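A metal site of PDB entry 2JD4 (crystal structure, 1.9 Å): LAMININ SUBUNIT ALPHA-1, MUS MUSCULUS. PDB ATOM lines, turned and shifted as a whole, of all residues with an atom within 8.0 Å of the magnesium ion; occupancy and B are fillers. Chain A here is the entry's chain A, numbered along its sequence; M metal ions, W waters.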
ATOM      1  N   ARG A  42      14.985  21.478   7.214  1.00  0.00           N
ATOM      2  CA  ARG A  42      14.045  21.680   8.308  1.00  0.00           C
ATOM      3  C   ARG A  42      13.830  20.435   9.182  1.00  0.00           C
ATOM      4  O   ARG A  42      13.871  20.521  10.406  1.00  0.00           O
ATOM      5  CB  ARG A  42      12.699  22.163   7.763  1.00  0.00           C
ATOM      6  CG  ARG A  42      12.732  23.592   7.223  1.00  0.00           C
ATOM      7  CD  ARG A  42      11.401  23.961   6.601  1.00  0.00           C
ATOM      8  NE  ARG A  42      11.129  23.180   5.393  1.00  0.00           N
ATOM      9  CZ  ARG A  42      10.011  23.281   4.675  1.00  0.00           C
ATOM     10  NH1 ARG A  42       9.060  24.121   5.047  1.00  0.00           N
ATOM     11  NH2 ARG A  42       9.853  22.531   3.588  1.00  0.00           N
ATOM     12  N   HIS A  65      20.186  30.632  11.381  1.00  0.00           N
ATOM     13  CA  HIS A  65      19.129  31.545  11.004  1.00  0.00           C
ATOM     14  C   HIS A  65      19.756  32.930  11.023  1.00  0.00           C
ATOM     15  O   HIS A  65      20.810  33.134  11.650  1.00  0.00           O
ATOM     16  CB  HIS A  65      17.986  31.441  12.013  1.00  0.00           C
ATOM     17  CG  HIS A  65      16.777  32.243  11.642  1.00  0.00           C
ATOM     18  ND1 HIS A  65      16.737  33.612  11.752  1.00  0.00           N
ATOM     19  CD2 HIS A  65      15.578  31.873  11.148  1.00  0.00           C
ATOM     20  CE1 HIS A  65      15.558  34.058  11.338  1.00  0.00           C
ATOM     21  NE2 HIS A  65      14.837  33.008  10.965  1.00  0.00           N
ATOM     22  N   MET A  69      18.794  32.208  16.110  1.00  0.00           N
ATOM     23  CA  MET A  69      18.004  31.465  17.087  1.00  0.00           C
ATOM     24  C   MET A  69      17.992  29.982  16.742  1.00  0.00           C
ATOM     25  O   MET A  69      17.703  29.145  17.593  1.00  0.00           O
ATOM     26  CB  MET A  69      16.572  32.026  17.130  1.00  0.00           C
ATOM     27  CG  MET A  69      16.180  32.610  18.479  1.00  0.00           C
ATOM     28  SD  MET A  69      17.434  33.693  19.191  1.00  0.00           S
ATOM     29  CE  MET A  69      17.116  35.242  18.307  1.00  0.00           C
ATOM     30  N   ASP A  70      18.297  29.668  15.486  1.00  0.00           N
ATOM     31  CA  ASP A  70      18.382  28.302  14.998  1.00  0.00           C
ATOM     32  C   ASP A  70      19.803  28.141  14.451  1.00  0.00           C
ATOM     33  O   ASP A  70      20.329  29.067  13.841  1.00  0.00           O
ATOM     34  CB  ASP A  70      17.385  28.059  13.845  1.00  0.00           C
ATOM     35  CG  ASP A  70      15.951  27.925  14.307  1.00  0.00           C
ATOM     36  OD1 ASP A  70      15.480  28.821  15.036  1.00  0.00           O
ATOM     37  OD2 ASP A  70      15.309  26.911  13.947  1.00  0.00           O
ATOM     38  N   TYR A  71      20.415  26.979  14.667  1.00  0.00           N
ATOM     39  CA  TYR A  71      21.768  26.750  14.146  1.00  0.00           C
ATOM     40  C   TYR A  71      22.170  25.288  14.213  1.00  0.00           C
ATOM     41  O   TYR A  71      21.504  24.469  14.843  1.00  0.00           O
ATOM     42  CB  TYR A  71      22.795  27.595  14.918  1.00  0.00           C
ATOM     43  CG  TYR A  71      22.951  27.205  16.378  1.00  0.00           C
ATOM     44  CD1 TYR A  71      23.597  26.034  16.739  1.00  0.00           C
ATOM     45  CD2 TYR A  71      22.406  28.003  17.393  1.00  0.00           C
ATOM     46  CE1 TYR A  71      23.701  25.641  18.082  1.00  0.00           C
ATOM     47  CE2 TYR A  71      22.506  27.627  18.738  1.00  0.00           C
ATOM     48  CZ  TYR A  71      23.161  26.443  19.073  1.00  0.00           C
ATOM     49  OH  TYR A  71      23.229  26.047  20.383  1.00  0.00           O
ATOM     50  N   ASP A  86      20.313  23.697  17.460  1.00  0.00           N
ATOM     51  CA  ASP A  86      19.204  24.201  18.259  1.00  0.00           C
ATOM     52  C   ASP A  86      18.089  24.516  17.262  1.00  0.00           C
ATOM     53  O   ASP A  86      18.282  25.319  16.342  1.00  0.00           O
ATOM     54  CB  ASP A  86      19.594  25.493  18.995  1.00  0.00           C
ATOM     55  CG  ASP A  86      18.617  25.851  20.109  1.00  0.00           C
ATOM     56  OD1 ASP A  86      17.397  25.656  19.928  1.00  0.00           O
ATOM     57  OD2 ASP A  86      19.081  26.367  21.154  1.00  0.00           O
ATOM     58  N   LEU A  87      16.932  23.892  17.440  1.00  0.00           N
ATOM     59  CA  LEU A  87      15.794  24.102  16.548  1.00  0.00           C
ATOM     60  C   LEU A  87      14.963  25.323  16.932  1.00  0.00           C
ATOM     61  O   LEU A  87      13.920  25.586  16.317  1.00  0.00           O
ATOM     62  CB  LEU A  87      14.909  22.859  16.528  1.00  0.00           C
ATOM     63  CG  LEU A  87      15.607  21.514  16.292  1.00  0.00           C
ATOM     64  CD1 LEU A  87      14.571  20.404  16.260  1.00  0.00           C
ATOM     65  CD2 LEU A  87      16.381  21.549  14.965  1.00  0.00           C
ATOM     66  N   GLY A  88      15.391  26.060  17.947  1.00  0.00           N
ATOM     67  CA  GLY A  88      14.655  27.242  18.358  1.00  0.00           C
ATOM     68  C   GLY A  88      14.189  27.264  19.806  1.00  0.00           C
ATOM     69  O   GLY A  88      13.810  28.318  20.320  1.00  0.00           O
ATOM     70  N   LYS A  89      14.209  26.109  20.469  1.00  0.00           N
ATOM     71  CA  LYS A  89      13.773  26.035  21.858  1.00  0.00           C
ATOM     72  C   LYS A  89      14.610  25.087  22.719  1.00  0.00           C
ATOM     73  O   LYS A  89      14.122  24.540  23.715  1.00  0.00           O
ATOM     74  CB  LYS A  89      12.294  25.624  21.919  1.00  0.00           C
ATOM     75  CG  LYS A  89      11.375  26.640  21.266  1.00  0.00           C
ATOM     76  CD  LYS A  89       9.937  26.167  21.259  1.00  0.00           C
ATOM     77  CE  LYS A  89       9.036  27.199  20.608  1.00  0.00           C
ATOM     78  NZ  LYS A  89       7.603  26.778  20.610  1.00  0.00           N
ATOM     79  N   TYR A 112      20.984  14.679  11.769  1.00  0.00           N
ATOM     80  CA  TYR A 112      19.834  15.114  12.540  1.00  0.00           C
ATOM     81  C   TYR A 112      18.675  14.633  11.672  1.00  0.00           C
ATOM     82  O   TYR A 112      18.541  15.063  10.526  1.00  0.00           O
ATOM     83  CB  TYR A 112      19.775  16.631  12.665  1.00  0.00           C
ATOM     84  CG  TYR A 112      18.356  17.188  12.718  1.00  0.00           C
ATOM     85  CD1 TYR A 112      17.431  16.714  13.648  1.00  0.00           C
ATOM     86  CD2 TYR A 112      17.954  18.179  11.826  1.00  0.00           C
ATOM     87  CE1 TYR A 112      16.116  17.216  13.673  1.00  0.00           C
ATOM     88  CE2 TYR A 112      16.644  18.695  11.850  1.00  0.00           C
ATOM     89  CZ  TYR A 112      15.731  18.200  12.775  1.00  0.00           C
ATOM     90  OH  TYR A 112      14.448  18.703  12.791  1.00  0.00           O
ATOM     91  N   ALA A 135      10.343  22.709  19.650  1.00  0.00           N
ATOM     92  CA  ALA A 135      10.467  23.132  18.259  1.00  0.00           C
ATOM     93  C   ALA A 135      10.665  21.893  17.392  1.00  0.00           C
ATOM     94  O   ALA A 135      11.202  20.885  17.854  1.00  0.00           O
ATOM     95  CB  ALA A 135      11.662  24.073  18.106  1.00  0.00           C
ATOM     96  N   THR A 136      10.216  21.963  16.141  1.00  0.00           N
ATOM     97  CA  THR A 136      10.340  20.801  15.257  1.00  0.00           C
ATOM     98  C   THR A 136      11.121  21.045  13.975  1.00  0.00           C
ATOM     99  O   THR A 136      11.356  20.108  13.215  1.00  0.00           O
ATOM    100  CB  THR A 136       8.948  20.274  14.847  1.00  0.00           C
ATOM    101  OG1 THR A 136       8.294  21.214  13.994  1.00  0.00           O
ATOM    102  CG2 THR A 136       8.083  20.038  16.073  1.00  0.00           C
ATOM    103  N   THR A 137      11.537  22.272  13.719  1.00  0.00           N
ATOM    104  CA  THR A 137      12.271  22.555  12.484  1.00  0.00           C
ATOM    105  C   THR A 137      13.579  23.329  12.651  1.00  0.00           C
ATOM    106  O   THR A 137      13.697  24.208  13.512  1.00  0.00           O
ATOM    107  CB  THR A 137      11.381  23.320  11.475  1.00  0.00           C
ATOM    108  OG1 THR A 137      11.057  24.614  11.999  1.00  0.00           O
ATOM    109  CG2 THR A 137      10.107  22.553  11.194  1.00  0.00           C
ATOM    110  N   LEU A 138      14.562  22.977  11.818  1.00  0.00           N
ATOM    111  CA  LEU A 138      15.851  23.666  11.809  1.00  0.00           C
ATOM    112  C   LEU A 138      15.684  24.701  10.703  1.00  0.00           C
ATOM    113  O   LEU A 138      15.730  24.365   9.528  1.00  0.00           O
ATOM    114  CB  LEU A 138      16.999  22.713  11.457  1.00  0.00           C
ATOM    115  CG  LEU A 138      18.364  23.350  11.198  1.00  0.00           C
ATOM    116  CD1 LEU A 138      18.903  24.000  12.486  1.00  0.00           C
ATOM    117  CD2 LEU A 138      19.339  22.280  10.695  1.00  0.00           C
ATOM    118  N   ASP A 139      15.469  25.945  11.108  1.00  0.00           N
ATOM    119  CA  ASP A 139      15.256  27.053  10.177  1.00  0.00           C
ATOM    120  C   ASP A 139      16.511  27.911  10.075  1.00  0.00           C
ATOM    121  O   ASP A 139      16.812  28.677  10.984  1.00  0.00           O
ATOM    122  CB  ASP A 139      14.080  27.905  10.651  1.00  0.00           C
ATOM    123  CG  ASP A 139      12.852  27.075  10.961  1.00  0.00           C
ATOM    124  OD1 ASP A 139      12.198  26.610  10.001  1.00  0.00           O
ATOM    125  OD2 ASP A 139      12.550  26.859  12.159  1.00  0.00           O
ATOM    126  N   VAL A 140      17.237  27.784   8.963  1.00  0.00           N
ATOM    127  CA  VAL A 140      18.468  28.546   8.783  1.00  0.00           C
ATOM    128  C   VAL A 140      18.616  29.111   7.376  1.00  0.00           C
ATOM    129  O   VAL A 140      17.938  28.673   6.440  1.00  0.00           O
ATOM    130  CB  VAL A 140      19.699  27.674   9.077  1.00  0.00           C
ATOM    131  CG1 VAL A 140      19.622  27.110  10.491  1.00  0.00           C
ATOM    132  CG2 VAL A 140      19.777  26.529   8.067  1.00  0.00           C
HETATM  133 MG    MG M   1      13.169  26.249  14.264  1.00  0.00          MG
HETATM  134  O   HOH W   1      12.886  28.390  15.159  1.00  0.00           O
HETATM  135  O   HOH W   2      11.121  25.539  14.846  1.00  0.00           O
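O of Asp 70 is in hydrogen-bond range of N of His 65 (2.9 Å).
Four residues have an atom within 4 Å of the magnesium ion: Asp 70, Leu 87, Thr 137 and Asp 139.
The magnesium ion is bound by the backbone carbonyl oxygen (O) of Thr 137 (2.2 Å). The magnesium ion is bound by water W2, 2.2 Å away. The magnesium ion is bound by OD2 of Asp 70. The magnesium ion is bound by OD2 of Asp 139 (2.3 Å). The magnesium ion is bound by O of Leu 87, at 2.3 Å. The magnesium ion is bound by water W1 (2.3 Å). The magnesium ion has six donor atoms within binding distance.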
